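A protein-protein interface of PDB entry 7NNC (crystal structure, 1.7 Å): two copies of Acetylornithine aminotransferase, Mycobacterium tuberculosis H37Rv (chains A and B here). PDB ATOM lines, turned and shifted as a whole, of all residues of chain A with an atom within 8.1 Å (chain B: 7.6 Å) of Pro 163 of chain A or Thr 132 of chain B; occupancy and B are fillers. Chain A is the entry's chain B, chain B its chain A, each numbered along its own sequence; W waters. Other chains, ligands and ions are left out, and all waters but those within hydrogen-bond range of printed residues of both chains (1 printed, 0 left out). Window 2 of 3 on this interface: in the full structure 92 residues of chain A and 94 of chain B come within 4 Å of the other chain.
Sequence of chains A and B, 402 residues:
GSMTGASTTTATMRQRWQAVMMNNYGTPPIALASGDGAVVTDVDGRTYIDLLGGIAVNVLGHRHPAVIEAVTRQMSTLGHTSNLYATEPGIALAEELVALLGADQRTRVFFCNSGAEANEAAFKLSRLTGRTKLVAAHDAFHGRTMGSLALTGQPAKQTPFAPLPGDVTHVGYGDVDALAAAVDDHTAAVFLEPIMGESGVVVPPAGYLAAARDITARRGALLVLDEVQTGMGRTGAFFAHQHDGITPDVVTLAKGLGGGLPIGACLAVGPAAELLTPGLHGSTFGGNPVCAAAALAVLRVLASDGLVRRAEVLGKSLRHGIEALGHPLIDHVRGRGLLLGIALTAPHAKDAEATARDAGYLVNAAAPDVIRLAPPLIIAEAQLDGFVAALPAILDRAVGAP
Water W1 lies within hydrogen-bond range of O of Pro 163 of chain A and N of Gly 166 of chain B.
The backbone carbonyl oxygen (O) of Thr 132 of chain B sits at hydrogen-bond distance from the guanidinium group (NH1) of Arg 127 of chain B. O of Gly 166 of chain B lies within hydrogen-bond range of NH2 of Arg 127 of chain B (2.8 Å). O of Phe 123 of chain B sits at hydrogen-bond distance from OG of Ser 126 of chain B. O of Thr 132 of chain B lies within hydrogen-bond range of N of Asp 167 of chain B (3.0 Å).
Among the printed residues, merely in contact across the chains: Met 146 of chain A with Phe 123 of chain B (3.7 Å), Pro 165 of chain A with Pro 165 of chain B (3.7 Å), Pro 160 of chain A with Arg 127 of chain B (3.8 Å), Ala 162 of chain A with Thr 132 of chain B (3.9 Å) and Pro 163 of chain A with Thr 132 of chain B (3.9 Å).
NH2 of Arg 127 of chain B sits at hydrogen-bond distance from O of Pro 163 of chain A (2.9 Å). The backbone carbonyl oxygen (O) of Phe 161 of chain A sits at hydrogen-bond distance from the guanidinium group (NE) of Arg 127 of chain B. NE of Arg 127 of chain B lies within hydrogen-bond range of O of Ala 162 of chain A (3.4 Å).
Hydrophobic or aromatic side chains of chain B within 4 Å of the printed part of chain A: Phe 123 and Pro 165. Along chain B the printed residues that touch a printed residue of chain A span positions 123 to 165. Among the printed residues, 8 pairs touch across the chains. Among the printed residues, no Asp or Glu carboxylate lies within 4 Å of a Lys or Arg side-chain nitrogen of the other chain.
Pro 165 of chain B touches its own counterpart, Pro 165 of chain A. Of the 8 pairs that touch across the chains among the printed residues, 1 has its exchanged pair printed and touching as well.
Thr 132 of chain B touches just these residues of chain A: Ala 162 (3.9 Å) and Pro 163 (3.9 Å). No residue of chain A comes within 4 Å of Lys 133 of chain B. Of the printed residues of chain B, Met 146 of chain A touches Phe 123. Of the printed residues of chain A, Pro 165 of chain B touches Pro 165 (3.7 Å). Printed residues of chain B within 4 Å of Pro 165 of chain A: Pro 165. Printed residues of chain B within 4 Å of Pro 160 of chain A: Arg 127 (3.8 Å). Of the printed residues of chain A, Arg 127 of chain B touches Pro 160 (3.8 Å), Phe 161 (2.8 Å), Ala 162 (3.4 Å) and Pro 163 (2.9 Å). Leu 164 of chain A touches none of the printed residues of chain B. The nearest residue of chain B that does not touch Pro 163 of chain A is Gly 166 of chain B (4.6 Å). The nearest residue of chain A that does not touch Thr 132 of chain B is Phe 161 of chain A (6.5 Å). The nearest printed residue of chain B that does not touch Pro 165 of chain A is Leu 164 of chain B (5.1 Å).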
ATOM      1  N   MET A 146     -32.307  29.028 -18.526  1.00  0.00           N
ATOM      2  CA  MET A 146     -31.559  29.964 -17.663  1.00  0.00           C
ATOM      3  C   MET A 146     -31.880  31.430 -17.945  1.00  0.00           C
ATOM      4  O   MET A 146     -31.998  32.229 -17.003  1.00  0.00           O
ATOM      5  CB  MET A 146     -30.058  29.695 -17.783  1.00  0.00           C
ATOM      6  CG  MET A 146     -29.557  28.384 -17.151  1.00  0.00           C
ATOM      7  SD  MET A 146     -29.868  28.298 -15.349  1.00  0.00           S
ATOM      8  CE  MET A 146     -28.637  29.485 -14.786  1.00  0.00           C
ATOM      9  N   ALA A 150     -34.380  33.866 -15.428  1.00  0.00           N
ATOM     10  CA  ALA A 150     -33.965  35.131 -14.828  1.00  0.00           C
ATOM     11  C   ALA A 150     -35.088  36.155 -14.879  1.00  0.00           C
ATOM     12  O   ALA A 150     -35.207  36.992 -13.980  1.00  0.00           O
ATOM     13  CB  ALA A 150     -32.726  35.674 -15.544  1.00  0.00           C
ATOM     14  N   GLN A 158     -35.987  30.098  -8.663  1.00  0.00           N
ATOM     15  CA  GLN A 158     -34.793  30.733  -9.250  1.00  0.00           C
ATOM     16  C   GLN A 158     -33.554  30.519  -8.381  1.00  0.00           C
ATOM     17  O   GLN A 158     -32.541  30.172  -8.904  1.00  0.00           O
ATOM     18  CB  GLN A 158     -34.985  32.241  -9.317  1.00  0.00           C
ATOM     19  CG  GLN A 158     -36.065  32.692 -10.268  1.00  0.00           C
ATOM     20  CD  GLN A 158     -36.191  34.195 -10.262  1.00  0.00           C
ATOM     21  OE1 GLN A 158     -36.599  34.763  -9.268  1.00  0.00           O
ATOM     22  NE2 GLN A 158     -35.805  34.847 -11.334  1.00  0.00           N
ATOM     23  N   THR A 159     -33.694  30.760  -7.085  1.00  0.00           N
ATOM     24  CA  THR A 159     -32.493  30.747  -6.205  1.00  0.00           C
ATOM     25  C   THR A 159     -31.700  29.436  -6.258  1.00  0.00           C
ATOM     26  O   THR A 159     -30.497  29.529  -6.253  1.00  0.00           O
ATOM     27  CB  THR A 159     -32.762  31.290  -4.802  1.00  0.00           C
ATOM     28  OG1 THR A 159     -33.653  30.350  -4.234  1.00  0.00           O
ATOM     29  CG2 THR A 159     -33.375  32.666  -4.841  1.00  0.00           C
ATOM     30  N   PRO A 160     -32.271  28.215  -6.378  1.00  0.00           N
ATOM     31  CA  PRO A 160     -31.432  27.014  -6.481  1.00  0.00           C
ATOM     32  C   PRO A 160     -30.468  26.981  -7.680  1.00  0.00           C
ATOM     33  O   PRO A 160     -29.544  26.252  -7.635  1.00  0.00           O
ATOM     34  CB  PRO A 160     -32.405  25.847  -6.633  1.00  0.00           C
ATOM     35  CG  PRO A 160     -33.706  26.364  -6.079  1.00  0.00           C
ATOM     36  CD  PRO A 160     -33.673  27.854  -6.315  1.00  0.00           C
ATOM     37  N   PHE A 161     -30.784  27.731  -8.734  1.00  0.00           N
ATOM     38  CA  PHE A 161     -30.003  27.799  -9.983  1.00  0.00           C
ATOM     39  C   PHE A 161     -29.119  29.046 -10.094  1.00  0.00           C
ATOM     40  O   PHE A 161     -28.512  29.212 -11.118  1.00  0.00           O
ATOM     41  CB  PHE A 161     -30.986  27.657 -11.144  1.00  0.00           C
ATOM     42  CG  PHE A 161     -31.877  26.465 -10.937  1.00  0.00           C
ATOM     43  CD1 PHE A 161     -31.380  25.193 -11.090  1.00  0.00           C
ATOM     44  CD2 PHE A 161     -33.175  26.592 -10.492  1.00  0.00           C
ATOM     45  CE1 PHE A 161     -32.171  24.090 -10.862  1.00  0.00           C
ATOM     46  CE2 PHE A 161     -33.968  25.484 -10.267  1.00  0.00           C
ATOM     47  CZ  PHE A 161     -33.464  24.232 -10.452  1.00  0.00           C
ATOM     48  N   ALA A 162     -29.030  29.845  -9.029  1.00  0.00           N
ATOM     49  CA  ALA A 162     -28.183  31.053  -9.032  1.00  0.00           C
ATOM     50  C   ALA A 162     -26.712  30.669  -9.214  1.00  0.00           C
ATOM     51  O   ALA A 162     -26.298  29.648  -8.731  1.00  0.00           O
ATOM     52  CB  ALA A 162     -28.367  31.829  -7.750  1.00  0.00           C
ATOM     53  N   PRO A 163     -25.898  31.502  -9.869  1.00  0.00           N
ATOM     54  CA  PRO A 163     -26.350  32.755 -10.456  1.00  0.00           C
ATOM     55  C   PRO A 163     -27.050  32.641 -11.823  1.00  0.00           C
ATOM     56  O   PRO A 163     -26.642  31.927 -12.630  1.00  0.00           O
ATOM     57  CB  PRO A 163     -25.021  33.487 -10.698  1.00  0.00           C
ATOM     58  CG  PRO A 163     -24.081  32.365 -11.022  1.00  0.00           C
ATOM     59  CD  PRO A 163     -24.478  31.298 -10.032  1.00  0.00           C
ATOM     60  N   LEU A 164     -28.083  33.452 -12.010  1.00  0.00           N
ATOM     61  CA  LEU A 164     -28.795  33.525 -13.306  1.00  0.00           C
ATOM     62  C   LEU A 164     -28.249  34.691 -14.127  1.00  0.00           C
ATOM     63  O   LEU A 164     -27.671  35.595 -13.560  1.00  0.00           O
ATOM     64  CB  LEU A 164     -30.294  33.735 -13.070  1.00  0.00           C
ATOM     65  CG  LEU A 164     -31.008  32.649 -12.270  1.00  0.00           C
ATOM     66  CD1 LEU A 164     -32.486  32.952 -12.130  1.00  0.00           C
ATOM     67  CD2 LEU A 164     -30.843  31.309 -12.909  1.00  0.00           C
ATOM     68  N   PRO A 165     -28.468  34.691 -15.452  1.00  0.00           N
ATOM     69  CA  PRO A 165     -28.028  35.776 -16.324  1.00  0.00           C
ATOM     70  C   PRO A 165     -28.533  37.148 -15.836  1.00  0.00           C
ATOM     71  O   PRO A 165     -29.641  37.237 -15.460  1.00  0.00           O
ATOM     72  CB  PRO A 165     -28.711  35.470 -17.660  1.00  0.00           C
ATOM     73  CG  PRO A 165     -29.199  34.073 -17.596  1.00  0.00           C
ATOM     74  CD  PRO A 165     -29.053  33.597 -16.177  1.00  0.00           C
ATOM     75  N   GLY A 166     -27.702  38.182 -15.932  1.00  0.00           N
ATOM     76  CA  GLY A 166     -28.101  39.508 -15.435  1.00  0.00           C
ATOM     77  C   GLY A 166     -28.613  40.444 -16.508  1.00  0.00           C
ATOM     78  O   GLY A 166     -28.615  40.068 -17.638  1.00  0.00           O
ATOM     79  N   PHE B 123     -27.663  21.841 -17.394  1.00  0.00           N
ATOM     80  CA  PHE B 123     -27.117  23.014 -16.717  1.00  0.00           C
ATOM     81  C   PHE B 123     -27.768  23.201 -15.353  1.00  0.00           C
ATOM     82  O   PHE B 123     -27.079  23.395 -14.342  1.00  0.00           O
ATOM     83  CB  PHE B 123     -27.338  24.249 -17.605  1.00  0.00           C
ATOM     84  CG  PHE B 123     -26.503  25.457 -17.232  1.00  0.00           C
ATOM     85  CD1 PHE B 123     -26.655  26.081 -15.993  1.00  0.00           C
ATOM     86  CD2 PHE B 123     -25.582  25.970 -18.128  1.00  0.00           C
ATOM     87  CE1 PHE B 123     -25.886  27.201 -15.662  1.00  0.00           C
ATOM     88  CE2 PHE B 123     -24.803  27.082 -17.809  1.00  0.00           C
ATOM     89  CZ  PHE B 123     -24.955  27.690 -16.569  1.00  0.00           C
ATOM     90  N   SER B 126     -26.683  20.653 -12.853  1.00  0.00           N
ATOM     91  CA  SER B 126     -25.320  21.006 -12.384  1.00  0.00           C
ATOM     92  C   SER B 126     -25.398  21.974 -11.196  1.00  0.00           C
ATOM     93  O   SER B 126     -24.580  21.890 -10.307  1.00  0.00           O
ATOM     94  CB  SER B 126     -24.483  21.609 -13.491  1.00  0.00           C
ATOM     95  OG  SER B 126     -24.600  23.008 -13.572  1.00  0.00           O
ATOM     96  N   ARG B 127     -26.350  22.896 -11.257  1.00  0.00           N
ATOM     97  CA  ARG B 127     -26.462  23.855 -10.162  1.00  0.00           C
ATOM     98  C   ARG B 127     -26.823  23.160  -8.857  1.00  0.00           C
ATOM     99  O   ARG B 127     -26.395  23.595  -7.777  1.00  0.00           O
ATOM    100  CB  ARG B 127     -27.513  24.915 -10.511  1.00  0.00           C
ATOM    101  CG  ARG B 127     -27.052  25.940 -11.557  1.00  0.00           C
ATOM    102  CD  ARG B 127     -26.135  26.990 -10.928  1.00  0.00           C
ATOM    103  NE  ARG B 127     -25.958  28.183 -11.756  1.00  0.00           N
ATOM    104  CZ  ARG B 127     -24.887  28.485 -12.494  1.00  0.00           C
ATOM    105  NH1 ARG B 127     -23.827  27.667 -12.583  1.00  0.00           N
ATOM    106  NH2 ARG B 127     -24.879  29.642 -13.154  1.00  0.00           N
ATOM    107  N   THR B 129     -25.828  20.476  -7.649  1.00  0.00           N
ATOM    108  CA  THR B 129     -24.690  19.863  -6.974  1.00  0.00           C
ATOM    109  C   THR B 129     -24.083  20.774  -5.922  1.00  0.00           C
ATOM    110  O   THR B 129     -23.166  20.345  -5.209  1.00  0.00           O
ATOM    111  CB  THR B 129     -23.580  19.516  -7.959  1.00  0.00           C
ATOM    112  OG1 THR B 129     -22.998  20.731  -8.469  1.00  0.00           O
ATOM    113  CG2 THR B 129     -24.133  18.682  -9.115  1.00  0.00           C
ATOM    114  N   GLY B 130     -24.530  22.028  -5.848  1.00  0.00           N
ATOM    115  CA  GLY B 130     -23.943  23.011  -4.964  1.00  0.00           C
ATOM    116  C   GLY B 130     -22.728  23.718  -5.518  1.00  0.00           C
ATOM    117  O   GLY B 130     -22.135  24.542  -4.815  1.00  0.00           O
ATOM    118  N   ARG B 131     -22.336  23.413  -6.749  1.00  0.00           N
ATOM    119  CA  ARG B 131     -21.178  23.977  -7.413  1.00  0.00           C
ATOM    120  C   ARG B 131     -21.641  24.804  -8.603  1.00  0.00           C
ATOM    121  O   ARG B 131     -22.685  24.520  -9.185  1.00  0.00           O
ATOM    122  CB  ARG B 131     -20.249  22.858  -7.888  1.00  0.00           C
ATOM    123  CG  ARG B 131     -19.734  21.972  -6.740  1.00  0.00           C
ATOM    124  CD  ARG B 131     -18.828  20.886  -7.310  1.00  0.00           C
ATOM    125  NE  ARG B 131     -18.383  19.945  -6.279  1.00  0.00           N
ATOM    126  CZ  ARG B 131     -17.394  19.075  -6.465  1.00  0.00           C
ATOM    127  NH1 ARG B 131     -16.772  19.038  -7.634  1.00  0.00           N
ATOM    128  NH2 ARG B 131     -17.034  18.246  -5.493  1.00  0.00           N
ATOM    129  N   THR B 132     -20.872  25.839  -8.956  1.00  0.00           N
ATOM    130  CA  THR B 132     -21.276  26.721 -10.049  1.00  0.00           C
ATOM    131  C   THR B 132     -20.266  26.802 -11.185  1.00  0.00           C
ATOM    132  O   THR B 132     -20.535  27.490 -12.174  1.00  0.00           O
ATOM    133  CB  THR B 132     -21.548  28.146  -9.543  1.00  0.00           C
ATOM    134  OG1 THR B 132     -20.364  28.679  -8.955  1.00  0.00           O
ATOM    135  CG2 THR B 132     -22.679  28.154  -8.520  1.00  0.00           C
ATOM    136  N   LYS B 133     -19.142  26.103 -11.075  1.00  0.00           N
ATOM    137  CA  LYS B 133     -18.086  26.146 -12.110  1.00  0.00           C
ATOM    138  C   LYS B 133     -18.365  25.049 -13.137  1.00  0.00           C
ATOM    139  O   LYS B 133     -18.679  23.957 -12.746  1.00  0.00           O
ATOM    140  CB  LYS B 133     -16.724  25.867 -11.475  1.00  0.00           C
ATOM    141  N   LEU B 134     -18.246  25.400 -14.413  1.00  0.00           N
ATOM    142  CA  LEU B 134     -18.501  24.461 -15.506  1.00  0.00           C
ATOM    143  C   LEU B 134     -17.320  24.451 -16.461  1.00  0.00           C
ATOM    144  O   LEU B 134     -16.627  25.459 -16.616  1.00  0.00           O
ATOM    145  CB  LEU B 134     -19.777  24.836 -16.270  1.00  0.00           C
ATOM    146  CG  LEU B 134     -21.009  24.808 -15.356  1.00  0.00           C
ATOM    147  CD1 LEU B 134     -22.092  25.766 -15.826  1.00  0.00           C
ATOM    148  CD2 LEU B 134     -21.536  23.392 -15.279  1.00  0.00           C
ATOM    149  N   VAL B 135     -17.101  23.310 -17.127  1.00  0.00           N
ATOM    150  CA  VAL B 135     -16.023  23.189 -18.107  1.00  0.00           C
ATOM    151  C   VAL B 135     -16.599  22.615 -19.399  1.00  0.00           C
ATOM    152  O   VAL B 135     -17.381  21.659 -19.374  1.00  0.00           O
ATOM    153  CB  VAL B 135     -14.870  22.299 -17.589  1.00  0.00           C
ATOM    154  CG1 VAL B 135     -13.809  22.119 -18.661  1.00  0.00           C
ATOM    155  CG2 VAL B 135     -14.252  22.868 -16.299  1.00  0.00           C
ATOM    156  N   LEU B 164     -23.115  36.097 -20.078  1.00  0.00           N
ATOM    157  CA  LEU B 164     -23.840  34.812 -20.090  1.00  0.00           C
ATOM    158  C   LEU B 164     -23.769  34.203 -18.692  1.00  0.00           C
ATOM    159  O   LEU B 164     -22.911  34.554 -17.944  1.00  0.00           O
ATOM    160  CB  LEU B 164     -23.194  33.862 -21.105  1.00  0.00           C
ATOM    161  CG  LEU B 164     -23.101  34.361 -22.544  1.00  0.00           C
ATOM    162  CD1 LEU B 164     -22.378  33.374 -23.409  1.00  0.00           C
ATOM    163  CD2 LEU B 164     -24.462  34.617 -23.121  1.00  0.00           C
ATOM    164  N   PRO B 165     -24.626  33.228 -18.381  1.00  0.00           N
ATOM    165  CA  PRO B 165     -24.583  32.505 -17.122  1.00  0.00           C
ATOM    166  C   PRO B 165     -23.166  31.935 -16.896  1.00  0.00           C
ATOM    167  O   PRO B 165     -22.601  31.403 -17.773  1.00  0.00           O
ATOM    168  CB  PRO B 165     -25.506  31.303 -17.389  1.00  0.00           C
ATOM    169  CG  PRO B 165     -26.417  31.738 -18.447  1.00  0.00           C
ATOM    170  CD  PRO B 165     -25.728  32.829 -19.222  1.00  0.00           C
ATOM    171  N   GLY B 166     -22.676  32.024 -15.667  1.00  0.00           N
ATOM    172  CA  GLY B 166     -21.327  31.515 -15.355  1.00  0.00           C
ATOM    173  C   GLY B 166     -21.338  30.206 -14.589  1.00  0.00           C
ATOM    174  O   GLY B 166     -22.376  29.670 -14.380  1.00  0.00           O
ATOM    175  N   ASP B 167     -20.174  29.715 -14.169  1.00  0.00           N
ATOM    176  CA  ASP B 167     -18.834  30.255 -14.496  1.00  0.00           C
ATOM    177  C   ASP B 167     -18.173  29.185 -15.353  1.00  0.00           C
ATOM    178  O   ASP B 167     -17.843  28.166 -14.832  1.00  0.00           O
ATOM    179  CB  ASP B 167     -18.018  30.445 -13.228  1.00  0.00           C
ATOM    180  CG  ASP B 167     -18.531  31.565 -12.356  1.00  0.00           C
ATOM    181  OD1 ASP B 167     -19.132  32.487 -12.897  1.00  0.00           O
ATOM    182  OD2 ASP B 167     -18.320  31.490 -11.148  1.00  0.00           O
ATOM    183  N   VAL B 168     -18.022  29.474 -16.636  1.00  0.00           N
ATOM    184  CA  VAL B 168     -17.577  28.424 -17.578  1.00  0.00           C
ATOM    185  C   VAL B 168     -16.155  28.658 -18.045  1.00  0.00           C
ATOM    186  O   VAL B 168     -15.870  29.730 -18.482  1.00  0.00           O
ATOM    187  CB  VAL B 168     -18.507  28.356 -18.798  1.00  0.00           C
ATOM    188  CG1 VAL B 168     -18.195  27.151 -19.659  1.00  0.00           C
ATOM    189  CG2 VAL B 168     -19.966  28.387 -18.379  1.00  0.00           C
ATOM    190  N   HIS B 186     -14.373  22.418  -7.201  1.00  0.00           N
ATOM    191  CA  HIS B 186     -15.432  23.397  -7.383  1.00  0.00           C
ATOM    192  C   HIS B 186     -16.201  23.219  -8.668  1.00  0.00           C
ATOM    193  O   HIS B 186     -17.130  23.994  -8.927  1.00  0.00           O
ATOM    194  CB  HIS B 186     -14.861  24.802  -7.334  1.00  0.00           C
ATOM    195  CG  HIS B 186     -14.167  25.090  -6.055  1.00  0.00           C
ATOM    196  ND1 HIS B 186     -14.809  24.942  -4.849  1.00  0.00           N
ATOM    197  CD2 HIS B 186     -12.887  25.418  -5.772  1.00  0.00           C
ATOM    198  CE1 HIS B 186     -13.974  25.243  -3.879  1.00  0.00           C
ATOM    199  NE2 HIS B 186     -12.794  25.515  -4.407  1.00  0.00           N
ATOM    200  N   THR B 187     -15.852  22.215  -9.464  1.00  0.00           N
ATOM    201  CA  THR B 187     -16.433  22.047 -10.786  1.00  0.00           C
ATOM    202  C   THR B 187     -17.723  21.242 -10.680  1.00  0.00           C
ATOM    203  O   THR B 187     -17.706  20.082 -10.258  1.00  0.00           O
ATOM    204  CB  THR B 187     -15.427  21.352 -11.706  1.00  0.00           C
ATOM    205  OG1 THR B 187     -14.256  22.174 -11.825  1.00  0.00           O
ATOM    206  CG2 THR B 187     -16.021  21.159 -13.090  1.00  0.00           C
ATOM    207  N   ALA B 188     -18.847  21.860 -11.063  1.00  0.00           N
ATOM    208  CA  ALA B 188     -20.120  21.150 -11.047  1.00  0.00           C
ATOM    209  C   ALA B 188     -20.165  20.067 -12.112  1.00  0.00           C
ATOM    210  O   ALA B 188     -20.663  18.961 -11.862  1.00  0.00           O
ATOM    211  CB  ALA B 188     -21.281  22.125 -11.259  1.00  0.00           C
ATOM    212  N   ALA B 189     -19.694  20.381 -13.315  1.00  0.00           N
ATOM    213  CA  ALA B 189     -19.896  19.468 -14.432  1.00  0.00           C
ATOM    214  C   ALA B 189     -18.955  19.819 -15.563  1.00  0.00           C
ATOM    215  O   ALA B 189     -18.582  20.983 -15.741  1.00  0.00           O
ATOM    216  CB  ALA B 189     -21.344  19.524 -14.940  1.00  0.00           C
HETATM  217  O   HOH W   1     -25.025  33.065 -14.246  1.00  0.00           O
